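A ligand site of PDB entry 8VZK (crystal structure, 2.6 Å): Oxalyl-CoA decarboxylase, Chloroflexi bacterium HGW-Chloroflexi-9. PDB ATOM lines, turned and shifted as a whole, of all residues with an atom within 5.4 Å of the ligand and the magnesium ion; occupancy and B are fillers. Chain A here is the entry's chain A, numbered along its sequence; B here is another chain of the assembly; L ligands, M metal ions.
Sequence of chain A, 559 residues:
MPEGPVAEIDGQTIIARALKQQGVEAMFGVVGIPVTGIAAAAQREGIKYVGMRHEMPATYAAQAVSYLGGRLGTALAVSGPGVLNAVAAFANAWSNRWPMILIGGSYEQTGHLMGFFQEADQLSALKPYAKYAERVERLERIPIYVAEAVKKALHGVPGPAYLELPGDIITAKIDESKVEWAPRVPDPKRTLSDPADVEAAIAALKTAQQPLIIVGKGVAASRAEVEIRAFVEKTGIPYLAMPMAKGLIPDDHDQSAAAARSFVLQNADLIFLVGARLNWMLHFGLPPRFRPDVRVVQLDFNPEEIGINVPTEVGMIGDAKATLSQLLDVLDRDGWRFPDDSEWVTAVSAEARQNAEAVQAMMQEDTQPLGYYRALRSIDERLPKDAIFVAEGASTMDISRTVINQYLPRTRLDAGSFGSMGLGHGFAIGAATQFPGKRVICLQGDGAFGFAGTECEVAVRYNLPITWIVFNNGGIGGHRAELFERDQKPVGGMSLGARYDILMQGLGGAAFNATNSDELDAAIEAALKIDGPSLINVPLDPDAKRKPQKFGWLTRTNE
The backbone NH (N) of Asp 446 sits close to an oxygen (O3) of the ligand. An oxygen (O7) of the ligand lies within hydrogen-bond range of the backbone NH (N) of Ser 395, at 2.8 Å. OG of Ser 395 sits at hydrogen-bond distance from O7 of the ligand, 2.4 Å away. An oxygen (O7) of the ligand sits at hydrogen-bond distance from the backbone NH (N) of Thr 396, 3.5 Å away. OG1 of Thr 396 sits at hydrogen-bond distance from O6 of the ligand, at 2.6 Å. A nitrogen (N3) of the ligand lies within hydrogen-bond range of the backbone carbonyl oxygen of Gly 419 (2.6 Å). OE2 of Glu 55 of chain B lies within hydrogen-bond range of N1 of the ligand. An oxygen (O3) of the ligand sits close to the backbone NH (N) of Gly 447, at 2.9 Å. OH of Tyr 372 lies within hydrogen-bond range of O6 of the ligand (2.9 Å). The backbone NH (N) of Met 421 sits at hydrogen-bond distance from a nitrogen (N2) of the ligand (3.1 Å). The backbone NH (N) of Gly 477 lies close to an oxygen (O5) of the ligand (3.1 Å). The backbone NH (N) of Ala 448 sits at hydrogen-bond distance from an oxygen (O2) of the ligand, at 3.2 Å. O4 of the ligand sits at hydrogen-bond distance from N of Ala 394 (3.4 Å). The side-chain amide nitrogen (NE2) of Gln 118 of chain B sits close to a nitrogen (N3) of the ligand, 3.4 Å away. An oxygen (O7) of the ligand is in salt-bridge range of the guanidinium group (NH2) of Arg 546 (3.6 Å).
OD1 of Asn 473 lies close to O of Gly 475 (3.2 Å). N of Gly 475 is in hydrogen-bond range of OD2 of Asp 446 (2.6 Å). N of Gly 474 lies within hydrogen-bond range of OD2 of Asp 446 (3.2 Å). OG of Ser 395 is in hydrogen-bond range of OH of Tyr 372 (2.9 Å). The side-chain hydroxyl of Ser 395 lies within hydrogen-bond range of the guanidinium group of Arg 546, 3.0 Å away. The side-chain amide nitrogen (NE2) of Gln 118 of chain B lies within hydrogen-bond range of the backbone carbonyl oxygen (O) of Gly 419, 3.3 Å away. The side-chain carboxylate of Glu 55 of chain B lies within hydrogen-bond range of the side-chain amide nitrogen of Asn 85 of chain B, at 3.1 Å. The backbone carbonyl oxygen of Gln 444 is in hydrogen-bond range of the backbone NH of Phe 471.
Residues that only touch the ligand: Gly 393 (3.2 Å), Val 31 of chain B (3.3 Å), Gly 445 (3.4 Å), Asn 85 of chain B (3.4 Å), Phe 451 (3.5 Å), Ile 476 (3.6 Å), Val 78 of chain B (3.6 Å), Pro 81 of chain B (3.6 Å), Val 30 of chain B (3.7 Å), Gly 82 of chain B (3.7 Å) and Ser 420 (3.9 Å). Of the 37 residues printed, 26 come within 4 Å of the ligand.
Merely in contact with the magnesium ion: Phe 471 (3.7 Å).
The magnesium ion is bound by OD1 of Asn 473. An oxygen (O3) of the ligand is bound to the magnesium ion (2.0 Å). OD1 of Asp 446 binds the magnesium ion. The magnesium ion is bound by an oxygen (O5) of the ligand (2.5 Å). The magnesium ion has four donor atoms within binding distance. Slightly farther from the magnesium ion lies the backbone carbonyl oxygen (O) of Gly 475 (2.6 Å). Slightly farther from the magnesium ion lies O6 of the ligand (2.8 Å).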
ATOM      1  N   TYR A 372      -2.022  23.730 -12.190  1.00  0.00           N
ATOM      2  CA  TYR A 372      -2.080  22.936 -13.412  1.00  0.00           C
ATOM      3  C   TYR A 372      -1.297  21.633 -13.252  1.00  0.00           C
ATOM      4  O   TYR A 372      -1.802  20.551 -13.551  1.00  0.00           O
ATOM      5  CB  TYR A 372      -1.540  23.738 -14.594  1.00  0.00           C
ATOM      6  CG  TYR A 372      -2.540  24.685 -15.216  1.00  0.00           C
ATOM      7  CD1 TYR A 372      -3.585  24.196 -15.994  1.00  0.00           C
ATOM      8  CD2 TYR A 372      -2.434  26.057 -15.044  1.00  0.00           C
ATOM      9  CE1 TYR A 372      -4.502  25.058 -16.577  1.00  0.00           C
ATOM     10  CE2 TYR A 372      -3.343  26.926 -15.624  1.00  0.00           C
ATOM     11  CZ  TYR A 372      -4.380  26.418 -16.382  1.00  0.00           C
ATOM     12  OH  TYR A 372      -5.285  27.278 -16.952  1.00  0.00           O
ATOM     13  N   GLU A 392      -9.387  19.616 -24.117  1.00  0.00           N
ATOM     14  CA  GLU A 392      -9.844  20.806 -24.827  1.00  0.00           C
ATOM     15  C   GLU A 392      -9.670  22.025 -23.945  1.00  0.00           C
ATOM     16  O   GLU A 392      -9.984  21.987 -22.760  1.00  0.00           O
ATOM     17  CB  GLU A 392     -11.316  20.671 -25.263  1.00  0.00           C
ATOM     18  CG  GLU A 392     -11.802  21.775 -26.188  1.00  0.00           C
ATOM     19  CD  GLU A 392     -13.296  21.711 -26.422  1.00  0.00           C
ATOM     20  OE1 GLU A 392     -14.053  21.443 -25.466  1.00  0.00           O
ATOM     21  OE2 GLU A 392     -13.724  21.935 -27.580  1.00  0.00           O
ATOM     22  N   GLY A 393      -9.157  23.094 -24.528  1.00  0.00           N
ATOM     23  CA  GLY A 393      -8.956  24.339 -23.822  1.00  0.00           C
ATOM     24  C   GLY A 393      -7.648  24.979 -24.236  1.00  0.00           C
ATOM     25  O   GLY A 393      -7.090  24.668 -25.288  1.00  0.00           O
ATOM     26  N   ALA A 394      -7.174  25.885 -23.389  1.00  0.00           N
ATOM     27  CA  ALA A 394      -5.898  26.560 -23.640  1.00  0.00           C
ATOM     28  C   ALA A 394      -4.780  25.856 -22.895  1.00  0.00           C
ATOM     29  O   ALA A 394      -4.325  24.785 -23.309  1.00  0.00           O
ATOM     30  CB  ALA A 394      -5.984  28.032 -23.229  1.00  0.00           C
ATOM     31  N   SER A 395      -4.317  26.457 -21.792  1.00  0.00           N
ATOM     32  CA  SER A 395      -3.237  25.853 -21.021  1.00  0.00           C
ATOM     33  C   SER A 395      -3.650  24.519 -20.400  1.00  0.00           C
ATOM     34  O   SER A 395      -2.806  23.640 -20.230  1.00  0.00           O
ATOM     35  CB  SER A 395      -2.768  26.831 -19.948  1.00  0.00           C
ATOM     36  OG  SER A 395      -3.857  27.597 -19.455  1.00  0.00           O
ATOM     37  N   THR A 396      -4.934  24.370 -20.068  1.00  0.00           N
ATOM     38  CA  THR A 396      -5.433  23.075 -19.607  1.00  0.00           C
ATOM     39  C   THR A 396      -5.131  21.990 -20.629  1.00  0.00           C
ATOM     40  O   THR A 396      -4.665  20.891 -20.277  1.00  0.00           O
ATOM     41  CB  THR A 396      -6.937  23.156 -19.347  1.00  0.00           C
ATOM     42  OG1 THR A 396      -7.187  24.030 -18.238  1.00  0.00           O
ATOM     43  CG2 THR A 396      -7.506  21.783 -19.037  1.00  0.00           C
ATOM     44  N   GLY A 419      -7.535  24.035 -33.935  1.00  0.00           N
ATOM     45  CA  GLY A 419      -7.616  24.707 -32.639  1.00  0.00           C
ATOM     46  C   GLY A 419      -9.039  25.055 -32.240  1.00  0.00           C
ATOM     47  O   GLY A 419      -9.274  26.108 -31.642  1.00  0.00           O
ATOM     48  N   SER A 420      -9.993  24.175 -32.543  1.00  0.00           N
ATOM     49  CA  SER A 420     -11.398  24.475 -32.354  1.00  0.00           C
ATOM     50  C   SER A 420     -11.836  24.221 -30.916  1.00  0.00           C
ATOM     51  O   SER A 420     -11.330  23.326 -30.237  1.00  0.00           O
ATOM     52  CB  SER A 420     -12.253  23.654 -33.310  1.00  0.00           C
ATOM     53  OG  SER A 420     -11.737  23.681 -34.625  1.00  0.00           O
ATOM     54  N   MET A 421     -12.786  25.032 -30.467  1.00  0.00           N
ATOM     55  CA  MET A 421     -13.495  24.793 -29.215  1.00  0.00           C
ATOM     56  C   MET A 421     -14.885  24.243 -29.513  1.00  0.00           C
ATOM     57  O   MET A 421     -15.447  24.478 -30.586  1.00  0.00           O
ATOM     58  CB  MET A 421     -13.609  26.072 -28.382  1.00  0.00           C
ATOM     59  CG  MET A 421     -12.300  26.561 -27.781  1.00  0.00           C
ATOM     60  SD  MET A 421     -11.597  25.429 -26.560  1.00  0.00           S
ATOM     61  CE  MET A 421     -10.158  24.824 -27.435  1.00  0.00           C
ATOM     62  N   GLN A 444     -11.274  19.257 -19.697  1.00  0.00           N
ATOM     63  CA  GLN A 444     -11.625  20.525 -20.319  1.00  0.00           C
ATOM     64  C   GLN A 444     -11.384  21.660 -19.350  1.00  0.00           C
ATOM     65  O   GLN A 444     -11.437  21.488 -18.133  1.00  0.00           O
ATOM     66  CB  GLN A 444     -13.087  20.551 -20.782  1.00  0.00           C
ATOM     67  CG  GLN A 444     -13.407  19.650 -21.966  1.00  0.00           C
ATOM     68  CD  GLN A 444     -14.894  19.612 -22.278  1.00  0.00           C
ATOM     69  OE1 GLN A 444     -15.715  19.340 -21.398  1.00  0.00           O
ATOM     70  NE2 GLN A 444     -15.238  19.899 -23.520  1.00  0.00           N
ATOM     71  N   GLY A 445     -11.113  22.844 -19.901  1.00  0.00           N
ATOM     72  CA  GLY A 445     -11.166  24.054 -19.115  1.00  0.00           C
ATOM     73  C   GLY A 445     -12.593  24.552 -18.986  1.00  0.00           C
ATOM     74  O   GLY A 445     -13.496  24.105 -19.694  1.00  0.00           O
ATOM     75  N   ASP A 446     -12.798  25.479 -18.057  1.00  0.00           N
ATOM     76  CA  ASP A 446     -14.143  26.009 -17.853  1.00  0.00           C
ATOM     77  C   ASP A 446     -14.632  26.759 -19.087  1.00  0.00           C
ATOM     78  O   ASP A 446     -15.817  26.681 -19.437  1.00  0.00           O
ATOM     79  CB  ASP A 446     -14.194  26.896 -16.614  1.00  0.00           C
ATOM     80  CG  ASP A 446     -13.077  27.920 -16.584  1.00  0.00           C
ATOM     81  OD1 ASP A 446     -12.040  27.685 -17.223  1.00  0.00           O
ATOM     82  OD2 ASP A 446     -13.249  28.963 -15.911  1.00  0.00           O
ATOM     83  N   GLY A 447     -13.739  27.475 -19.764  1.00  0.00           N
ATOM     84  CA  GLY A 447     -14.128  28.164 -20.983  1.00  0.00           C
ATOM     85  C   GLY A 447     -14.500  27.198 -22.094  1.00  0.00           C
ATOM     86  O   GLY A 447     -15.489  27.403 -22.795  1.00  0.00           O
ATOM     87  N   ALA A 448     -13.722  26.133 -22.255  1.00  0.00           N
ATOM     88  CA  ALA A 448     -14.028  25.135 -23.283  1.00  0.00           C
ATOM     89  C   ALA A 448     -15.307  24.384 -22.961  1.00  0.00           C
ATOM     90  O   ALA A 448     -16.067  24.029 -23.871  1.00  0.00           O
ATOM     91  CB  ALA A 448     -12.856  24.158 -23.434  1.00  0.00           C
ATOM     92  N   PHE A 449     -15.571  24.147 -21.677  1.00  0.00           N
ATOM     93  CA  PHE A 449     -16.732  23.354 -21.281  1.00  0.00           C
ATOM     94  C   PHE A 449     -18.053  24.042 -21.640  1.00  0.00           C
ATOM     95  O   PHE A 449     -19.041  23.366 -21.944  1.00  0.00           O
ATOM     96  CB  PHE A 449     -16.679  23.063 -19.775  1.00  0.00           C
ATOM     97  CG  PHE A 449     -17.846  22.273 -19.255  1.00  0.00           C
ATOM     98  CD1 PHE A 449     -17.846  20.890 -19.321  1.00  0.00           C
ATOM     99  CD2 PHE A 449     -18.937  22.912 -18.687  1.00  0.00           C
ATOM    100  CE1 PHE A 449     -18.917  20.149 -18.845  1.00  0.00           C
ATOM    101  CE2 PHE A 449     -20.007  22.184 -18.208  1.00  0.00           C
ATOM    102  CZ  PHE A 449     -19.999  20.795 -18.284  1.00  0.00           C
ATOM    103  N   PHE A 451     -19.007  25.633 -24.235  1.00  0.00           N
ATOM    104  CA  PHE A 451     -19.443  25.606 -25.625  1.00  0.00           C
ATOM    105  C   PHE A 451     -20.538  24.576 -25.858  1.00  0.00           C
ATOM    106  O   PHE A 451     -21.370  24.743 -26.765  1.00  0.00           O
ATOM    107  CB  PHE A 451     -18.254  25.337 -26.545  1.00  0.00           C
ATOM    108  CG  PHE A 451     -17.353  26.522 -26.741  1.00  0.00           C
ATOM    109  CD1 PHE A 451     -16.376  26.822 -25.818  1.00  0.00           C
ATOM    110  CD2 PHE A 451     -17.487  27.334 -27.862  1.00  0.00           C
ATOM    111  CE1 PHE A 451     -15.541  27.916 -25.990  1.00  0.00           C
ATOM    112  CE2 PHE A 451     -16.665  28.430 -28.047  1.00  0.00           C
ATOM    113  CZ  PHE A 451     -15.686  28.720 -27.105  1.00  0.00           C
ATOM    114  N   PHE A 471     -11.405  22.386 -15.266  1.00  0.00           N
ATOM    115  CA  PHE A 471     -10.526  23.280 -14.512  1.00  0.00           C
ATOM    116  C   PHE A 471     -11.151  24.668 -14.519  1.00  0.00           C
ATOM    117  O   PHE A 471     -11.018  25.420 -15.493  1.00  0.00           O
ATOM    118  CB  PHE A 471      -9.125  23.303 -15.114  1.00  0.00           C
ATOM    119  CG  PHE A 471      -8.326  22.044 -14.872  1.00  0.00           C
ATOM    120  CD1 PHE A 471      -8.862  21.003 -14.136  1.00  0.00           C
ATOM    121  CD2 PHE A 471      -7.050  21.919 -15.378  1.00  0.00           C
ATOM    122  CE1 PHE A 471      -8.126  19.846 -13.915  1.00  0.00           C
ATOM    123  CE2 PHE A 471      -6.314  20.762 -15.158  1.00  0.00           C
ATOM    124  CZ  PHE A 471      -6.856  19.728 -14.422  1.00  0.00           C
ATOM    125  N   ASN A 472     -11.836  25.019 -13.429  1.00  0.00           N
ATOM    126  CA  ASN A 472     -12.440  26.340 -13.295  1.00  0.00           C
ATOM    127  C   ASN A 472     -11.369  27.289 -12.759  1.00  0.00           C
ATOM    128  O   ASN A 472     -11.172  27.422 -11.554  1.00  0.00           O
ATOM    129  CB  ASN A 472     -13.653  26.281 -12.375  1.00  0.00           C
ATOM    130  CG  ASN A 472     -14.452  27.579 -12.363  1.00  0.00           C
ATOM    131  OD1 ASN A 472     -13.891  28.670 -12.288  1.00  0.00           O
ATOM    132  ND2 ASN A 472     -15.773  27.456 -12.450  1.00  0.00           N
ATOM    133  N   ASN A 473     -10.668  27.951 -13.685  1.00  0.00           N
ATOM    134  CA  ASN A 473      -9.636  28.911 -13.332  1.00  0.00           C
ATOM    135  C   ASN A 473     -10.062  30.359 -13.553  1.00  0.00           C
ATOM    136  O   ASN A 473      -9.239  31.266 -13.402  1.00  0.00           O
ATOM    137  CB  ASN A 473      -8.352  28.636 -14.126  1.00  0.00           C
ATOM    138  CG  ASN A 473      -8.513  28.917 -15.607  1.00  0.00           C
ATOM    139  OD1 ASN A 473      -9.607  28.813 -16.157  1.00  0.00           O
ATOM    140  ND2 ASN A 473      -7.416  29.296 -16.261  1.00  0.00           N
ATOM    141  N   GLY A 474     -11.323  30.605 -13.918  1.00  0.00           N
ATOM    142  CA  GLY A 474     -11.805  31.942 -14.137  1.00  0.00           C
ATOM    143  C   GLY A 474     -12.236  32.265 -15.561  1.00  0.00           C
ATOM    144  O   GLY A 474     -12.567  33.426 -15.831  1.00  0.00           O
ATOM    145  N   GLY A 475     -12.254  31.289 -16.466  1.00  0.00           N
ATOM    146  CA  GLY A 475     -12.705  31.496 -17.828  1.00  0.00           C
ATOM    147  C   GLY A 475     -11.569  31.322 -18.820  1.00  0.00           C
ATOM    148  O   GLY A 475     -10.629  30.536 -18.604  1.00  0.00           O
ATOM    149  N   ILE A 476     -11.663  32.064 -19.931  1.00  0.00           N
ATOM    150  CA  ILE A 476     -10.664  32.033 -20.987  1.00  0.00           C
ATOM    151  C   ILE A 476      -9.376  32.656 -20.454  1.00  0.00           C
ATOM    152  O   ILE A 476      -9.076  33.825 -20.741  1.00  0.00           O
ATOM    153  CB  ILE A 476     -11.165  32.760 -22.247  1.00  0.00           C
ATOM    154  CG1 ILE A 476     -12.604  32.349 -22.547  1.00  0.00           C
ATOM    155  CG2 ILE A 476     -10.270  32.457 -23.437  1.00  0.00           C
ATOM    156  CD1 ILE A 476     -13.324  33.288 -23.488  1.00  0.00           C
ATOM    157  N   GLY A 477      -8.624  31.887 -19.700  1.00  0.00           N
ATOM    158  CA  GLY A 477      -7.493  32.394 -18.941  1.00  0.00           C
ATOM    159  C   GLY A 477      -7.818  32.504 -17.458  1.00  0.00           C
ATOM    160  O   GLY A 477      -8.976  32.540 -17.040  1.00  0.00           O
ATOM    161  N   GLY A 478      -6.758  32.543 -16.655  1.00  0.00           N
ATOM    162  CA  GLY A 478      -6.910  32.611 -15.220  1.00  0.00           C
ATOM    163  C   GLY A 478      -7.208  34.006 -14.715  1.00  0.00           C
ATOM    164  O   GLY A 478      -6.309  34.855 -14.646  1.00  0.00           O
ATOM    165  N   LEU A 540      -9.525  25.715  -9.860  1.00  0.00           N
ATOM    166  CA  LEU A 540      -8.118  25.900 -10.168  1.00  0.00           C
ATOM    167  C   LEU A 540      -7.638  27.256  -9.683  1.00  0.00           C
ATOM    168  O   LEU A 540      -8.398  28.216  -9.594  1.00  0.00           O
ATOM    169  CB  LEU A 540      -7.879  25.757 -11.676  1.00  0.00           C
ATOM    170  CG  LEU A 540      -6.445  25.556 -12.145  1.00  0.00           C
ATOM    171  CD1 LEU A 540      -5.884  24.248 -11.603  1.00  0.00           C
ATOM    172  CD2 LEU A 540      -6.383  25.566 -13.663  1.00  0.00           C
ATOM    173  N   ARG A 546       1.942  28.327 -15.634  1.00  0.00           N
ATOM    174  CA  ARG A 546       1.704  27.568 -16.852  1.00  0.00           C
ATOM    175  C   ARG A 546       2.984  27.152 -17.563  1.00  0.00           C
ATOM    176  O   ARG A 546       2.918  26.527 -18.628  1.00  0.00           O
ATOM    177  CB  ARG A 546       0.820  28.386 -17.806  1.00  0.00           C
ATOM    178  CG  ARG A 546      -0.653  28.422 -17.410  1.00  0.00           C
ATOM    179  CD  ARG A 546      -1.190  29.841 -17.434  1.00  0.00           C
ATOM    180  NE  ARG A 546      -2.510  29.924 -18.052  1.00  0.00           N
ATOM    181  CZ  ARG A 546      -3.642  30.122 -17.399  1.00  0.00           C
ATOM    182  NH1 ARG A 546      -3.673  30.256 -16.082  1.00  0.00           N
ATOM    183  NH2 ARG A 546      -4.781  30.193 -18.081  1.00  0.00           N
ATOM    184  N   VAL B  30     -16.980  35.635 -27.854  1.00  0.00           N
ATOM    185  CA  VAL B  30     -16.094  34.730 -27.119  1.00  0.00           C
ATOM    186  C   VAL B  30     -14.688  35.021 -27.600  1.00  0.00           C
ATOM    187  O   VAL B  30     -14.334  34.720 -28.750  1.00  0.00           O
ATOM    188  CB  VAL B  30     -16.461  33.260 -27.355  1.00  0.00           C
ATOM    189  CG1 VAL B  30     -15.515  32.353 -26.596  1.00  0.00           C
ATOM    190  CG2 VAL B  30     -17.907  32.997 -26.942  1.00  0.00           C
ATOM    191  N   VAL B  31     -13.869  35.615 -26.735  1.00  0.00           N
ATOM    192  CA  VAL B  31     -12.581  36.149 -27.148  1.00  0.00           C
ATOM    193  C   VAL B  31     -11.545  35.046 -27.337  1.00  0.00           C
ATOM    194  O   VAL B  31     -11.812  33.864 -27.075  1.00  0.00           O
ATOM    195  CB  VAL B  31     -12.065  37.200 -26.147  1.00  0.00           C
ATOM    196  CG1 VAL B  31     -12.670  38.549 -26.465  1.00  0.00           C
ATOM    197  CG2 VAL B  31     -12.404  36.781 -24.719  1.00  0.00           C
ATOM    198  N   GLY B  32     -10.366  35.438 -27.795  1.00  0.00           N
ATOM    199  CA  GLY B  32      -9.339  34.498 -28.192  1.00  0.00           C
ATOM    200  C   GLY B  32      -8.509  35.114 -29.301  1.00  0.00           C
ATOM    201  O   GLY B  32      -8.779  36.209 -29.783  1.00  0.00           O
ATOM    202  N   ILE B  33      -7.476  34.372 -29.690  1.00  0.00           N
ATOM    203  CA  ILE B  33      -6.595  34.864 -30.763  1.00  0.00           C
ATOM    204  C   ILE B  33      -7.395  34.945 -32.058  1.00  0.00           C
ATOM    205  O   ILE B  33      -8.059  33.961 -32.442  1.00  0.00           O
ATOM    206  CB  ILE B  33      -5.377  33.936 -30.927  1.00  0.00           C
ATOM    207  CG1 ILE B  33      -4.500  33.991 -29.678  1.00  0.00           C
ATOM    208  CG2 ILE B  33      -4.588  34.318 -32.171  1.00  0.00           C
ATOM    209  CD1 ILE B  33      -3.260  33.123 -29.777  1.00  0.00           C
ATOM    210  N   GLU B  55     -20.328  31.091 -29.740  1.00  0.00           N
ATOM    211  CA  GLU B  55     -20.519  32.134 -30.750  1.00  0.00           C
ATOM    212  C   GLU B  55     -21.954  32.194 -31.254  1.00  0.00           C
ATOM    213  O   GLU B  55     -22.435  33.280 -31.611  1.00  0.00           O
ATOM    214  CB  GLU B  55     -19.559  31.924 -31.922  1.00  0.00           C
ATOM    215  CG  GLU B  55     -18.148  32.438 -31.677  1.00  0.00           C
ATOM    216  CD  GLU B  55     -17.239  31.403 -31.047  1.00  0.00           C
ATOM    217  OE1 GLU B  55     -17.622  30.219 -30.989  1.00  0.00           O
ATOM    218  OE2 GLU B  55     -16.141  31.790 -30.602  1.00  0.00           O
ATOM    219  N   VAL B  78     -13.828  34.605 -32.865  1.00  0.00           N
ATOM    220  CA  VAL B  78     -12.469  34.150 -33.096  1.00  0.00           C
ATOM    221  C   VAL B  78     -12.315  33.697 -34.542  1.00  0.00           C
ATOM    222  O   VAL B  78     -13.290  33.283 -35.200  1.00  0.00           O
ATOM    223  CB  VAL B  78     -12.126  33.024 -32.093  1.00  0.00           C
ATOM    224  CG1 VAL B  78     -10.789  32.353 -32.401  1.00  0.00           C
ATOM    225  CG2 VAL B  78     -12.109  33.576 -30.676  1.00  0.00           C
ATOM    226  N   PRO B  81     -12.756  28.585 -36.468  1.00  0.00           N
ATOM    227  CA  PRO B  81     -13.922  27.955 -35.833  1.00  0.00           C
ATOM    228  C   PRO B  81     -14.874  28.944 -35.184  1.00  0.00           C
ATOM    229  O   PRO B  81     -16.086  28.684 -35.141  1.00  0.00           O
ATOM    230  CB  PRO B  81     -13.296  27.023 -34.789  1.00  0.00           C
ATOM    231  CG  PRO B  81     -11.913  26.765 -35.288  1.00  0.00           C
ATOM    232  CD  PRO B  81     -11.484  28.018 -35.990  1.00  0.00           C
ATOM    233  N   GLY B  82     -14.372  30.074 -34.683  1.00  0.00           N
ATOM    234  CA  GLY B  82     -15.250  31.032 -34.021  1.00  0.00           C
ATOM    235  C   GLY B  82     -16.268  31.638 -34.974  1.00  0.00           C
ATOM    236  O   GLY B  82     -17.458  31.667 -34.678  1.00  0.00           O
ATOM    237  N   ASN B  85     -18.815  29.144 -36.245  1.00  0.00           N
ATOM    238  CA  ASN B  85     -19.759  28.675 -35.235  1.00  0.00           C
ATOM    239  C   ASN B  85     -21.067  29.457 -35.236  1.00  0.00           C
ATOM    240  O   ASN B  85     -22.004  29.054 -34.558  1.00  0.00           O
ATOM    241  CB  ASN B  85     -19.120  28.751 -33.852  1.00  0.00           C
ATOM    242  CG  ASN B  85     -18.871  27.386 -33.246  1.00  0.00           C
ATOM    243  OD1 ASN B  85     -19.035  26.368 -33.901  1.00  0.00           O
ATOM    244  ND2 ASN B  85     -18.464  27.370 -31.982  1.00  0.00           N
ATOM    245  N   PHE B 117      -2.384  29.622 -37.856  1.00  0.00           N
ATOM    246  CA  PHE B 117      -3.364  29.174 -36.873  1.00  0.00           C
ATOM    247  C   PHE B 117      -4.770  29.584 -37.290  1.00  0.00           C
ATOM    248  O   PHE B 117      -5.058  30.773 -37.443  1.00  0.00           O
ATOM    249  CB  PHE B 117      -3.021  29.757 -35.500  1.00  0.00           C
ATOM    250  CG  PHE B 117      -3.963  29.333 -34.411  1.00  0.00           C
ATOM    251  CD1 PHE B 117      -4.003  28.021 -33.989  1.00  0.00           C
ATOM    252  CD2 PHE B 117      -4.796  30.261 -33.805  1.00  0.00           C
ATOM    253  CE1 PHE B 117      -4.865  27.631 -32.981  1.00  0.00           C
ATOM    254  CE2 PHE B 117      -5.651  29.877 -32.793  1.00  0.00           C
ATOM    255  CZ  PHE B 117      -5.696  28.560 -32.384  1.00  0.00           C
ATOM    256  N   GLN B 118      -5.628  28.581 -37.495  1.00  0.00           N
ATOM    257  CA  GLN B 118      -7.026  28.792 -37.886  1.00  0.00           C
ATOM    258  C   GLN B 118      -7.137  29.508 -39.233  1.00  0.00           C
ATOM    259  O   GLN B 118      -8.093  30.240 -39.470  1.00  0.00           O
ATOM    260  CB  GLN B 118      -7.809  29.541 -36.805  1.00  0.00           C
ATOM    261  CG  GLN B 118      -7.877  28.793 -35.484  1.00  0.00           C
ATOM    262  CD  GLN B 118      -8.554  29.604 -34.391  1.00  0.00           C
ATOM    263  OE1 GLN B 118      -8.519  30.830 -34.401  1.00  0.00           O
ATOM    264  NE2 GLN B 118      -9.175  28.904 -33.451  1.00  0.00           N
HETATM  265  N1  LIG L   1     -14.248  29.733 -30.287  1.00  0.00           N
HETATM  266  C1  LIG L   1     -13.968  28.611 -30.966  1.00  0.00           C
HETATM  267  C2  LIG L   1     -15.090  27.946 -31.683  1.00  0.00           C
HETATM  268  N2  LIG L   1     -12.755  28.044 -31.051  1.00  0.00           N
HETATM  269  C3  LIG L   1     -11.740  28.643 -30.409  1.00  0.00           C
HETATM  270  N3  LIG L   1     -10.536  28.056 -30.498  1.00  0.00           N
HETATM  271  C4  LIG L   1     -11.941  29.835 -29.660  1.00  0.00           C
HETATM  272  C5  LIG L   1     -13.226  30.312 -29.657  1.00  0.00           C
HETATM  273  C6  LIG L   1     -10.833  30.540 -28.920  1.00  0.00           C
HETATM  274  N4  LIG L   1     -10.357  29.777 -27.733  1.00  0.00           N
HETATM  275  C7  LIG L   1      -9.301  28.996 -27.748  1.00  0.00           C
HETATM  276  S1  LIG L   1      -9.032  28.261 -26.264  1.00  0.00           S
HETATM  277  C8  LIG L   1     -10.415  29.043 -25.588  1.00  0.00           C
HETATM  278  C9  LIG L   1     -11.019  29.819 -26.514  1.00  0.00           C
HETATM  279  C10 LIG L   1     -12.236  30.658 -26.331  1.00  0.00           C
HETATM  280  C11 LIG L   1     -10.811  28.822 -24.157  1.00  0.00           C
HETATM  281  C12 LIG L   1      -9.628  28.645 -23.231  1.00  0.00           C
HETATM  282  O1  LIG L   1     -10.119  28.601 -21.870  1.00  0.00           O
HETATM  283  P1  LIG L   1     -10.110  27.316 -20.957  1.00  0.00           P
HETATM  284  O2  LIG L   1     -10.590  26.138 -21.719  1.00  0.00           O
HETATM  285  O3  LIG L   1     -10.890  27.625 -19.688  1.00  0.00           O
HETATM  286  O4  LIG L   1      -8.585  27.170 -20.548  1.00  0.00           O
HETATM  287  P2  LIG L   1      -7.592  27.649 -19.400  1.00  0.00           P
HETATM  288  O5  LIG L   1      -7.963  28.999 -18.886  1.00  0.00           O
HETATM  289  O6  LIG L   1      -7.691  26.542 -18.332  1.00  0.00           O
HETATM  290  O7  LIG L   1      -6.215  27.586 -20.039  1.00  0.00           O
HETATM  291 MG    MG M   1     -10.035  28.052 -17.906  1.00  0.00          MG
